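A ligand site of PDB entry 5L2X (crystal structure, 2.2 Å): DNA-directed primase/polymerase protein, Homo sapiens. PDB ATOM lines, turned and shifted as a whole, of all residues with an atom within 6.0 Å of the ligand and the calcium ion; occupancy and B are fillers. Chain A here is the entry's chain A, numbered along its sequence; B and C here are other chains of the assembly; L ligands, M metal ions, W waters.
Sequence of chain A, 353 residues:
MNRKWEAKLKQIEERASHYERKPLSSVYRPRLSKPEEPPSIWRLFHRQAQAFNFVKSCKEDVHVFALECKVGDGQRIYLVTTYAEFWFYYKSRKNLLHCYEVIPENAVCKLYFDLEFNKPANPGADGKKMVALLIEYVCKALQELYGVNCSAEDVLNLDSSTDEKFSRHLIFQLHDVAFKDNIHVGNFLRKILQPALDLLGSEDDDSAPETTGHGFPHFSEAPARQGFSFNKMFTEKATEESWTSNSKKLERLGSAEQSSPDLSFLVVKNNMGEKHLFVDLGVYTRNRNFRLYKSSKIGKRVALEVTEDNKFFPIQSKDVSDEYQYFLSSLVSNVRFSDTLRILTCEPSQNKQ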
ATOM      1  N   GLU A  68      20.231 -27.041  16.307  1.00  0.00           N
ATOM      2  CA  GLU A  68      21.642 -27.405  16.296  1.00  0.00           C
ATOM      3  C   GLU A  68      21.774 -28.920  16.232  1.00  0.00           C
ATOM      4  O   GLU A  68      21.308 -29.632  17.126  1.00  0.00           O
ATOM      5  CB  GLU A  68      22.330 -26.865  17.548  1.00  0.00           C
ATOM      6  CG  GLU A  68      23.001 -25.519  17.365  1.00  0.00           C
ATOM      7  CD  GLU A  68      23.842 -25.164  18.573  1.00  0.00           C
ATOM      8  OE1 GLU A  68      23.486 -25.612  19.690  1.00  0.00           O
ATOM      9  OE2 GLU A  68      24.855 -24.440  18.424  1.00  0.00           O
ATOM     10  N   GLY A  74      28.425 -25.172  14.920  1.00  0.00           N
ATOM     11  CA  GLY A  74      27.206 -24.406  15.053  1.00  0.00           C
ATOM     12  C   GLY A  74      26.300 -24.636  13.869  1.00  0.00           C
ATOM     13  O   GLY A  74      25.382 -23.845  13.605  1.00  0.00           O
ATOM     14  N   ARG A  76      23.351 -25.824  11.595  1.00  0.00           N
ATOM     15  CA  ARG A  76      21.939 -25.916  11.898  1.00  0.00           C
ATOM     16  C   ARG A  76      21.202 -26.572  10.738  1.00  0.00           C
ATOM     17  O   ARG A  76      21.626 -26.501   9.586  1.00  0.00           O
ATOM     18  CB  ARG A  76      21.310 -24.551  12.158  1.00  0.00           C
ATOM     19  CG  ARG A  76      21.619 -23.963  13.525  1.00  0.00           C
ATOM     20  CD  ARG A  76      22.344 -22.646  13.397  1.00  0.00           C
ATOM     21  NE  ARG A  76      22.107 -21.808  14.552  1.00  0.00           N
ATOM     22  CZ  ARG A  76      22.844 -21.828  15.661  1.00  0.00           C
ATOM     23  NH1 ARG A  76      23.863 -22.665  15.748  1.00  0.00           N
ATOM     24  NH2 ARG A  76      22.548 -21.023  16.672  1.00  0.00           N
ATOM     25  N   TYR A 100      16.462 -22.831  18.350  1.00  0.00           N
ATOM     26  CA  TYR A 100      16.671 -21.398  18.164  1.00  0.00           C
ATOM     27  C   TYR A 100      15.497 -20.811  17.389  1.00  0.00           C
ATOM     28  O   TYR A 100      15.022 -21.396  16.413  1.00  0.00           O
ATOM     29  CB  TYR A 100      17.994 -21.128  17.418  1.00  0.00           C
ATOM     30  CG  TYR A 100      19.210 -21.522  18.236  1.00  0.00           C
ATOM     31  CD1 TYR A 100      19.655 -22.833  18.255  1.00  0.00           C
ATOM     32  CD2 TYR A 100      19.873 -20.573  19.014  1.00  0.00           C
ATOM     33  CE1 TYR A 100      20.745 -23.198  19.014  1.00  0.00           C
ATOM     34  CE2 TYR A 100      20.971 -20.927  19.776  1.00  0.00           C
ATOM     35  CZ  TYR A 100      21.397 -22.250  19.761  1.00  0.00           C
ATOM     36  OH  TYR A 100      22.493 -22.629  20.518  1.00  0.00           O
ATOM     37  N   ASP A 114      20.477  -9.399  24.844  1.00  0.00           N
ATOM     38  CA  ASP A 114      21.369 -10.485  25.233  1.00  0.00           C
ATOM     39  C   ASP A 114      22.442  -9.866  26.120  1.00  0.00           C
ATOM     40  O   ASP A 114      23.279  -9.089  25.631  1.00  0.00           O
ATOM     41  CB  ASP A 114      21.969 -11.184  24.021  1.00  0.00           C
ATOM     42  CG  ASP A 114      22.891 -12.326  24.399  1.00  0.00           C
ATOM     43  OD1 ASP A 114      22.439 -13.204  25.161  1.00  0.00           O
ATOM     44  OD2 ASP A 114      24.054 -12.348  23.943  1.00  0.00           O
ATOM     45  N   LEU A 115      22.393 -10.160  27.423  1.00  0.00           N
ATOM     46  CA  LEU A 115      23.290  -9.581  28.416  1.00  0.00           C
ATOM     47  C   LEU A 115      24.215 -10.675  28.944  1.00  0.00           C
ATOM     48  O   LEU A 115      23.752 -11.751  29.330  1.00  0.00           O
ATOM     49  CB  LEU A 115      22.500  -8.966  29.564  1.00  0.00           C
ATOM     50  CG  LEU A 115      21.356  -8.050  29.165  1.00  0.00           C
ATOM     51  CD1 LEU A 115      20.562  -7.580  30.360  1.00  0.00           C
ATOM     52  CD2 LEU A 115      21.890  -6.854  28.372  1.00  0.00           C
ATOM     53  N   GLU A 116      25.505 -10.393  28.992  1.00  0.00           N
ATOM     54  CA  GLU A 116      26.454 -11.368  29.519  1.00  0.00           C
ATOM     55  C   GLU A 116      27.742 -10.688  29.980  1.00  0.00           C
ATOM     56  O   GLU A 116      28.152  -9.666  29.436  1.00  0.00           O
ATOM     57  CB  GLU A 116      26.793 -12.428  28.460  1.00  0.00           C
ATOM     58  CG  GLU A 116      27.354 -11.868  27.188  1.00  0.00           C
ATOM     59  CD  GLU A 116      27.464 -12.933  26.120  1.00  0.00           C
ATOM     60  OE1 GLU A 116      28.520 -13.059  25.473  1.00  0.00           O
ATOM     61  OE2 GLU A 116      26.472 -13.668  25.946  1.00  0.00           O
ATOM     62  N   SER A 160      20.386 -17.914  31.819  1.00  0.00           N
ATOM     63  CA  SER A 160      21.162 -19.067  31.401  1.00  0.00           C
ATOM     64  C   SER A 160      22.537 -19.066  32.053  1.00  0.00           C
ATOM     65  O   SER A 160      23.509 -19.512  31.453  1.00  0.00           O
ATOM     66  CB  SER A 160      21.295 -19.124  29.887  1.00  0.00           C
ATOM     67  OG  SER A 160      21.803 -20.387  29.486  1.00  0.00           O
ATOM     68  N   SER A 161      22.641 -18.535  33.264  1.00  0.00           N
ATOM     69  CA  SER A 161      23.932 -18.328  33.890  1.00  0.00           C
ATOM     70  C   SER A 161      24.576 -19.645  34.355  1.00  0.00           C
ATOM     71  O   SER A 161      23.895 -20.616  34.686  1.00  0.00           O
ATOM     72  CB  SER A 161      23.794 -17.372  35.072  1.00  0.00           C
ATOM     73  OG  SER A 161      23.379 -16.098  34.632  1.00  0.00           O
ATOM     74  N   LYS A 165      29.756 -17.688  33.721  1.00  0.00           N
ATOM     75  CA  LYS A 165      29.098 -16.672  32.898  1.00  0.00           C
ATOM     76  C   LYS A 165      27.779 -16.230  33.514  1.00  0.00           C
ATOM     77  O   LYS A 165      26.921 -17.058  33.815  1.00  0.00           O
ATOM     78  CB  LYS A 165      28.861 -17.208  31.479  1.00  0.00           C
ATOM     79  CG  LYS A 165      28.483 -16.145  30.467  1.00  0.00           C
ATOM     80  CD  LYS A 165      28.520 -16.718  29.055  1.00  0.00           C
ATOM     81  CE  LYS A 165      28.115 -15.678  28.006  1.00  0.00           C
ATOM     82  NZ  LYS A 165      27.965 -16.260  26.644  1.00  0.00           N
ATOM     83  N   SER A 167      24.587 -14.841  32.318  1.00  0.00           N
ATOM     84  CA  SER A 167      23.933 -14.810  31.005  1.00  0.00           C
ATOM     85  C   SER A 167      22.438 -14.608  31.185  1.00  0.00           C
ATOM     86  O   SER A 167      21.784 -15.416  31.848  1.00  0.00           O
ATOM     87  CB  SER A 167      24.215 -16.094  30.232  1.00  0.00           C
ATOM     88  OG  SER A 167      23.437 -16.162  29.062  1.00  0.00           O
ATOM     89  N   ARG A 168      21.905 -13.546  30.582  1.00  0.00           N
ATOM     90  CA  ARG A 168      20.481 -13.287  30.651  1.00  0.00           C
ATOM     91  C   ARG A 168      19.924 -12.810  29.323  1.00  0.00           C
ATOM     92  O   ARG A 168      20.585 -12.076  28.578  1.00  0.00           O
ATOM     93  CB  ARG A 168      20.155 -12.290  31.772  1.00  0.00           C
ATOM     94  CG  ARG A 168      20.202 -12.978  33.160  1.00  0.00           C
ATOM     95  CD  ARG A 168      19.360 -12.298  34.211  1.00  0.00           C
ATOM     96  NE  ARG A 168      19.794 -12.652  35.560  1.00  0.00           N
ATOM     97  CZ  ARG A 168      19.428 -11.978  36.647  1.00  0.00           C
ATOM     98  NH1 ARG A 168      18.615 -10.904  36.550  1.00  0.00           N
ATOM     99  NH2 ARG A 168      19.870 -12.366  37.831  1.00  0.00           N
ATOM    100  N   HIS A 169      18.715 -13.254  29.012  1.00  0.00           N
ATOM    101  CA  HIS A 169      17.959 -12.766  27.865  1.00  0.00           C
ATOM    102  C   HIS A 169      16.766 -11.991  28.405  1.00  0.00           C
ATOM    103  O   HIS A 169      16.017 -12.510  29.238  1.00  0.00           O
ATOM    104  CB  HIS A 169      17.470 -13.915  26.972  1.00  0.00           C
ATOM    105  CG  HIS A 169      18.549 -14.521  26.125  1.00  0.00           C
ATOM    106  ND1 HIS A 169      18.275 -15.376  25.086  1.00  0.00           N
ATOM    107  CD2 HIS A 169      19.897 -14.399  26.167  1.00  0.00           C
ATOM    108  CE1 HIS A 169      19.411 -15.753  24.508  1.00  0.00           C
ATOM    109  NE2 HIS A 169      20.412 -15.178  25.154  1.00  0.00           N
ATOM    110  N   ASP A 280      25.179  -7.083  24.728  1.00  0.00           N
ATOM    111  CA  ASP A 280      25.766  -7.656  23.517  1.00  0.00           C
ATOM    112  C   ASP A 280      25.096  -7.030  22.293  1.00  0.00           C
ATOM    113  O   ASP A 280      23.929  -7.303  22.003  1.00  0.00           O
ATOM    114  CB  ASP A 280      25.577  -9.167  23.569  1.00  0.00           C
ATOM    115  CG  ASP A 280      25.948  -9.871  22.277  1.00  0.00           C
ATOM    116  OD1 ASP A 280      26.493  -9.245  21.351  1.00  0.00           O
ATOM    117  OD2 ASP A 280      25.663 -11.086  22.205  1.00  0.00           O
ATOM    118  N   VAL A 283      23.689  -9.096  18.282  1.00  0.00           N
ATOM    119  CA  VAL A 283      22.530  -9.952  18.047  1.00  0.00           C
ATOM    120  C   VAL A 283      21.438  -9.258  17.247  1.00  0.00           C
ATOM    121  O   VAL A 283      20.354  -9.826  17.081  1.00  0.00           O
ATOM    122  CB  VAL A 283      21.948 -10.443  19.386  1.00  0.00           C
ATOM    123  CG1 VAL A 283      22.990 -11.209  20.155  1.00  0.00           C
ATOM    124  CG2 VAL A 283      21.480  -9.274  20.197  1.00  0.00           C
ATOM    125  N   ARG A 288      18.871 -13.242  12.704  1.00  0.00           N
ATOM    126  CA  ARG A 288      19.548 -13.656  13.929  1.00  0.00           C
ATOM    127  C   ARG A 288      18.871 -14.853  14.590  1.00  0.00           C
ATOM    128  O   ARG A 288      17.660 -14.879  14.784  1.00  0.00           O
ATOM    129  CB  ARG A 288      19.616 -12.475  14.910  1.00  0.00           C
ATOM    130  CG  ARG A 288      19.819 -12.901  16.369  1.00  0.00           C
ATOM    131  CD  ARG A 288      21.244 -13.314  16.664  1.00  0.00           C
ATOM    132  NE  ARG A 288      22.234 -12.600  15.843  1.00  0.00           N
ATOM    133  CZ  ARG A 288      23.532 -12.848  15.817  1.00  0.00           C
ATOM    134  NH1 ARG A 288      24.047 -13.790  16.597  1.00  0.00           N
ATOM    135  NH2 ARG A 288      24.298 -12.125  15.020  1.00  0.00           N
ATOM    136  N   ASN A 289      19.652 -15.878  14.897  1.00  0.00           N
ATOM    137  CA  ASN A 289      19.176 -16.996  15.711  1.00  0.00           C
ATOM    138  C   ASN A 289      19.157 -16.574  17.165  1.00  0.00           C
ATOM    139  O   ASN A 289      20.111 -15.956  17.646  1.00  0.00           O
ATOM    140  CB  ASN A 289      20.066 -18.218  15.529  1.00  0.00           C
ATOM    141  CG  ASN A 289      19.767 -18.974  14.260  1.00  0.00           C
ATOM    142  OD1 ASN A 289      20.145 -20.127  14.112  1.00  0.00           O
ATOM    143  ND2 ASN A 289      19.058 -18.326  13.329  1.00  0.00           N
ATOM    144  N   PHE A 290      18.066 -16.903  17.881  1.00  0.00           N
ATOM    145  CA  PHE A 290      17.974 -16.572  19.304  1.00  0.00           C
ATOM    146  C   PHE A 290      17.442 -17.786  20.060  1.00  0.00           C
ATOM    147  O   PHE A 290      16.348 -18.267  19.765  1.00  0.00           O
ATOM    148  CB  PHE A 290      17.084 -15.357  19.545  1.00  0.00           C
ATOM    149  CG  PHE A 290      17.494 -14.530  20.746  1.00  0.00           C
ATOM    150  CD1 PHE A 290      18.793 -14.073  20.859  1.00  0.00           C
ATOM    151  CD2 PHE A 290      16.595 -14.216  21.736  1.00  0.00           C
ATOM    152  CE1 PHE A 290      19.179 -13.306  21.947  1.00  0.00           C
ATOM    153  CE2 PHE A 290      16.980 -13.458  22.828  1.00  0.00           C
ATOM    154  CZ  PHE A 290      18.274 -12.994  22.930  1.00  0.00           C
ATOM    155  N   ARG A 291      18.214 -18.242  21.043  1.00  0.00           N
ATOM    156  CA  ARG A 291      18.000 -19.538  21.681  1.00  0.00           C
ATOM    157  C   ARG A 291      16.675 -19.568  22.414  1.00  0.00           C
ATOM    158  O   ARG A 291      16.344 -18.652  23.173  1.00  0.00           O
ATOM    159  CB  ARG A 291      19.179 -19.837  22.617  1.00  0.00           C
ATOM    160  CG  ARG A 291      19.077 -21.145  23.392  1.00  0.00           C
ATOM    161  CD  ARG A 291      20.450 -21.649  23.902  1.00  0.00           C
ATOM    162  NE  ARG A 291      21.106 -20.681  24.765  1.00  0.00           N
ATOM    163  CZ  ARG A 291      21.200 -20.754  26.095  1.00  0.00           C
ATOM    164  NH1 ARG A 291      20.688 -21.773  26.773  1.00  0.00           N
ATOM    165  NH2 ARG A 291      21.831 -19.782  26.742  1.00  0.00           N
ATOM    166  N   LYS A 297      22.573 -24.660  24.561  1.00  0.00           N
ATOM    167  CA  LYS A 297      23.546 -24.865  23.499  1.00  0.00           C
ATOM    168  C   LYS A 297      24.011 -26.312  23.498  1.00  0.00           C
ATOM    169  O   LYS A 297      24.043 -26.986  24.532  1.00  0.00           O
ATOM    170  CB  LYS A 297      24.735 -23.922  23.694  1.00  0.00           C
ATOM    171  CG  LYS A 297      24.421 -22.464  23.398  1.00  0.00           C
ATOM    172  CD  LYS A 297      25.481 -21.556  23.989  1.00  0.00           C
ATOM    173  CE  LYS A 297      25.830 -20.454  23.018  1.00  0.00           C
ATOM    174  NZ  LYS A 297      27.053 -19.704  23.434  1.00  0.00           N
ATOM    175  N   LEU A 304      17.791 -21.873  29.023  1.00  0.00           N
ATOM    176  CA  LEU A 304      17.200 -20.617  29.448  1.00  0.00           C
ATOM    177  C   LEU A 304      15.928 -20.894  30.248  1.00  0.00           C
ATOM    178  O   LEU A 304      15.097 -21.706  29.835  1.00  0.00           O
ATOM    179  CB  LEU A 304      16.902 -19.716  28.243  1.00  0.00           C
ATOM    180  CG  LEU A 304      18.116 -18.960  27.649  1.00  0.00           C
ATOM    181  CD1 LEU A 304      17.911 -18.725  26.165  1.00  0.00           C
ATOM    182  CD2 LEU A 304      18.404 -17.640  28.371  1.00  0.00           C
ATOM    183  P    DT B   3      27.070 -25.995   6.727  1.00  0.00           P
ATOM    184  OP1  DT B   3      27.519 -24.782   6.007  1.00  0.00           O
ATOM    185  OP2  DT B   3      28.058 -26.854   7.420  1.00  0.00           O
ATOM    186  O5'  DT B   3      25.971 -25.511   7.782  1.00  0.00           O
ATOM    187  C5'  DT B   3      24.583 -25.624   7.482  1.00  0.00           C
ATOM    188  C4'  DT B   3      23.833 -24.395   7.951  1.00  0.00           C
ATOM    189  O4'  DT B   3      24.302 -24.002   9.255  1.00  0.00           O
ATOM    190  C3'  DT B   3      23.996 -23.171   7.046  1.00  0.00           C
ATOM    191  O3'  DT B   3      22.719 -22.741   6.608  1.00  0.00           O
ATOM    192  C2'  DT B   3      24.711 -22.131   7.917  1.00  0.00           C
ATOM    193  C1'  DT B   3      24.419 -22.597   9.329  1.00  0.00           C
ATOM    194  N1   DT B   3      25.500 -22.280  10.340  1.00  0.00           N
ATOM    195  C2   DT B   3      25.278 -21.325  11.321  1.00  0.00           C
ATOM    196  O2   DT B   3      24.255 -20.679  11.421  1.00  0.00           O
ATOM    197  N3   DT B   3      26.322 -21.148  12.186  1.00  0.00           N
ATOM    198  C4   DT B   3      27.533 -21.808  12.181  1.00  0.00           C
ATOM    199  O4   DT B   3      28.410 -21.576  13.002  1.00  0.00           O
ATOM    200  C5   DT B   3      27.694 -22.792  11.139  1.00  0.00           C
ATOM    201  C7   DT B   3      28.978 -23.580  11.035  1.00  0.00           C
ATOM    202  C6   DT B   3      26.683 -22.979  10.289  1.00  0.00           C
ATOM    203  P    DC B   4      22.600 -21.700   5.392  1.00  0.00           P
ATOM    204  OP1  DC B   4      21.221 -21.744   4.839  1.00  0.00           O
ATOM    205  OP2  DC B   4      23.758 -21.912   4.508  1.00  0.00           O
ATOM    206  O5'  DC B   4      22.822 -20.299   6.094  1.00  0.00           O
ATOM    207  C5'  DC B   4      21.937 -19.886   7.084  1.00  0.00           C
ATOM    208  C4'  DC B   4      22.475 -18.677   7.817  1.00  0.00           C
ATOM    209  O4'  DC B   4      23.638 -19.028   8.588  1.00  0.00           O
ATOM    210  C3'  DC B   4      22.916 -17.505   6.936  1.00  0.00           C
ATOM    211  O3'  DC B   4      21.917 -16.476   7.024  1.00  0.00           O
ATOM    212  C2'  DC B   4      24.282 -17.071   7.550  1.00  0.00           C
ATOM    213  C1'  DC B   4      24.277 -17.822   8.879  1.00  0.00           C
ATOM    214  N1   DC B   4      25.606 -18.118   9.523  1.00  0.00           N
ATOM    215  C2   DC B   4      25.983 -17.417  10.681  1.00  0.00           C
ATOM    216  O2   DC B   4      25.231 -16.535  11.129  1.00  0.00           O
ATOM    217  N3   DC B   4      27.171 -17.732  11.279  1.00  0.00           N
ATOM    218  C4   DC B   4      27.947 -18.690  10.775  1.00  0.00           C
ATOM    219  N4   DC B   4      29.096 -18.947  11.406  1.00  0.00           N
ATOM    220  C5   DC B   4      27.584 -19.414   9.597  1.00  0.00           C
ATOM    221  C6   DC B   4      26.406 -19.114   9.022  1.00  0.00           C
ATOM    222  P   DDG C  13      31.603 -13.494  20.645  1.00  0.00           P
ATOM    223  OP1 DDG C  13      32.111 -12.574  21.728  1.00  0.00           O
ATOM    224  OP2 DDG C  13      31.842 -14.933  21.045  1.00  0.00           O
ATOM    225  O5' DDG C  13      30.008 -13.281  20.523  1.00  0.00           O
ATOM    226  C5' DDG C  13      29.422 -12.012  20.242  1.00  0.00           C
ATOM    227  C4' DDG C  13      28.073 -12.296  19.595  1.00  0.00           C
ATOM    228  O4' DDG C  13      28.274 -12.880  18.300  1.00  0.00           O
ATOM    229  C3' DDG C  13      27.311 -13.324  20.438  1.00  0.00           C
ATOM    230  C2' DDG C  13      26.851 -14.389  19.450  1.00  0.00           C
ATOM    231  C1' DDG C  13      27.317 -13.922  18.086  1.00  0.00           C
ATOM    232  N9  DDG C  13      27.974 -15.016  17.343  1.00  0.00           N
ATOM    233  C8  DDG C  13      29.045 -15.725  17.747  1.00  0.00           C
ATOM    234  N7  DDG C  13      29.399 -16.634  16.798  1.00  0.00           N
ATOM    235  C5  DDG C  13      28.552 -16.514  15.761  1.00  0.00           C
ATOM    236  C6  DDG C  13      28.370 -17.138  14.441  1.00  0.00           C
ATOM    237  O6  DDG C  13      29.118 -18.050  14.048  1.00  0.00           O
ATOM    238  N1  DDG C  13      27.362 -16.704  13.670  1.00  0.00           N
ATOM    239  C2  DDG C  13      26.532 -15.717  14.047  1.00  0.00           C
ATOM    240  N2  DDG C  13      25.534 -15.333  13.197  1.00  0.00           N
ATOM    241  N3  DDG C  13      26.656 -15.091  15.252  1.00  0.00           N
ATOM    242  C4  DDG C  13      27.621 -15.437  16.121  1.00  0.00           C
HETATM  243  P1  LIG L   1      25.030 -17.850  26.374  1.00  0.00           P
HETATM  244  O1  LIG L   1      26.160 -18.778  26.078  1.00  0.00           O
HETATM  245  O2  LIG L   1      25.395 -16.378  26.310  1.00  0.00           O
HETATM  246  O3  LIG L   1      24.297 -18.061  27.672  1.00  0.00           O
HETATM  247  P2  LIG L   1      23.399 -17.389  24.079  1.00  0.00           P
HETATM  248  O4  LIG L   1      22.132 -18.094  23.647  1.00  0.00           O
HETATM  249  O5  LIG L   1      23.166 -16.024  24.642  1.00  0.00           O
HETATM  250  O6  LIG L   1      23.999 -18.325  25.238  1.00  0.00           O
HETATM  251  P3  LIG L   1      25.411 -16.310  22.427  1.00  0.00           P
HETATM  252  O7  LIG L   1      26.729 -16.876  22.044  1.00  0.00           O
HETATM  253  O8  LIG L   1      25.482 -15.330  23.577  1.00  0.00           O
HETATM  254  O9  LIG L   1      24.432 -17.490  22.860  1.00  0.00           O
HETATM  255  O10 LIG L   1      24.741 -15.665  21.099  1.00  0.00           O
HETATM  256  C1  LIG L   1      23.431 -15.141  21.109  1.00  0.00           C
HETATM  257  C2  LIG L   1      22.625 -15.766  19.962  1.00  0.00           C
HETATM  258  O11 LIG L   1      23.291 -15.649  18.698  1.00  0.00           O
HETATM  259  C3  LIG L   1      22.422 -17.245  20.171  1.00  0.00           C
HETATM  260  O12 LIG L   1      21.292 -17.496  21.013  1.00  0.00           O
HETATM  261  C4  LIG L   1      22.220 -17.768  18.770  1.00  0.00           C
HETATM  262  C5  LIG L   1      23.054 -16.808  17.909  1.00  0.00           C
HETATM  263  N1  LIG L   1      24.292 -17.546  17.582  1.00  0.00           N
HETATM  264  C6  LIG L   1      25.356 -17.750  18.387  1.00  0.00           C
HETATM  265  N2  LIG L   1      26.296 -18.502  17.769  1.00  0.00           N
HETATM  266  C7  LIG L   1      25.809 -18.795  16.549  1.00  0.00           C
HETATM  267  C8  LIG L   1      26.286 -19.560  15.386  1.00  0.00           C
HETATM  268  N3  LIG L   1      27.509 -20.157  15.423  1.00  0.00           N
HETATM  269  N4  LIG L   1      25.493 -19.621  14.298  1.00  0.00           N
HETATM  270  C9  LIG L   1      24.294 -19.020  14.254  1.00  0.00           C
HETATM  271  N5  LIG L   1      23.795 -18.313  15.286  1.00  0.00           N
HETATM  272  C10 LIG L   1      24.501 -18.171  16.417  1.00  0.00           C
HETATM  273 CA    CA M   1      24.527 -14.372  25.360  1.00  0.00          CA
HETATM  274  O   HOH W   1      24.947 -20.867  28.266  1.00  0.00           O
HETATM  275  O   HOH W   2      23.591 -14.046  27.427  1.00  0.00           O
HETATM  276  O   HOH W   3      22.350 -16.144  14.306  1.00  0.00           O
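Water W2 lies within hydrogen-bond range of OG of Ser 167 and O of Leu 115.
Water W3 lies within hydrogen-bond range of N of Asn 289 (2.8 Å), N5 of the ligand (2.8 Å) and N2 of DDG 13 of chain C (3.5 Å).
Water W1 lies within hydrogen-bond range of O3 of the ligand (2.9 Å) and OG of Ser 160 (3.4 Å).
The side-chain carboxylate (OE1) of Glu 116 is in salt-bridge range of the side-chain amino group (NZ) of Lys 165, at 3.5 Å.
The side-chain carboxylate (OD1) of Asp 114 lies close to a ring nitrogen (NE2) of His 169, 2.8 Å away.
The backbone carbonyl oxygen (O) of Asp 114 sits at hydrogen-bond distance from the backbone NH (N) of Asp 280 (2.9 Å).
N of Ser 167 is in hydrogen-bond range of OG of Ser 161.
NH1 of Arg 288 lies within hydrogen-bond range of N3 of DDG 13 of chain C (3.2 Å).
O2 of DC 4 of chain B sits close to N2 of DDG 13 of chain C, 2.4 Å away.
OE2 of Glu 68 is in salt-bridge range of NH1 of Arg 76 (3.4 Å).
The side-chain hydroxyl (OH) of Tyr 100 lies within hydrogen-bond range of the side-chain carboxylate (OE1) of Glu 68 (3.3 Å).
The calcium ion is bound by the side-chain carboxylate (OE2) of Glu 116 (2.1 Å), an oxygen (O8) of the ligand (2.2 Å), an oxygen (O5) of the ligand (2.3 Å), water W2 (2.3 Å), an oxygen (O2) of the ligand (2.4 Å), the side-chain carboxylate (OD1) of Asp 114 (2.4 Å) and the side-chain carboxylate (OD2) of Asp 114 (2.5 Å).
An oxygen (O3) of the ligand lies within hydrogen-bond range of the side-chain hydroxyl (OG) of Ser 167, at 2.5 Å.
The side-chain amino group (NZ) of Lys 165 is in salt-bridge range of an oxygen (O1) of the ligand (3.1 Å).
O4 of DT 3 of chain B is in hydrogen-bond range of a nitrogen (N3) of the ligand (2.9 Å).
An oxygen (O11) of the ligand is in hydrogen-bond range of the guanidinium group (NH1) of Arg 288 (2.9 Å).
NE2 of His 169 sits close to O5 of the ligand.
NZ of Lys 297 lies within salt-bridge range of O1 of the ligand (2.9 Å).
A nitrogen (N3) of the ligand is in hydrogen-bond range of O6 of DDG 13 of chain C.
O12 of the ligand sits at hydrogen-bond distance from N of Arg 291 (3.2 Å).
An oxygen (O4) of the ligand lies within salt-bridge range of the guanidinium group (NE) of Arg 291, at 3.0 Å.
N5 of the ligand is in hydrogen-bond range of NH2 of Arg 76 (3.3 Å).
Two residues have an atom within 4 Å of the calcium ion: Asp 114 and Glu 116.
The nearest printed residue that does not touch the calcium ion is Lys 165 (4.1 Å).
An oxygen (O11) of the ligand sits close to the backbone carbonyl oxygen (O) of Asn 289 (3.4 Å).
Merely in contact with the ligand: Tyr 100 (3.5 Å), Phe 290 (3.8 Å), Ser 160 (3.9 Å) and DC 4 of chain B (3.9 Å).
Hydrophobic or aromatic side chains within 4 Å of the ligand: Tyr 100 and His 169.
The nearest printed residue that does not touch the ligand is Val 283 (4.1 Å).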
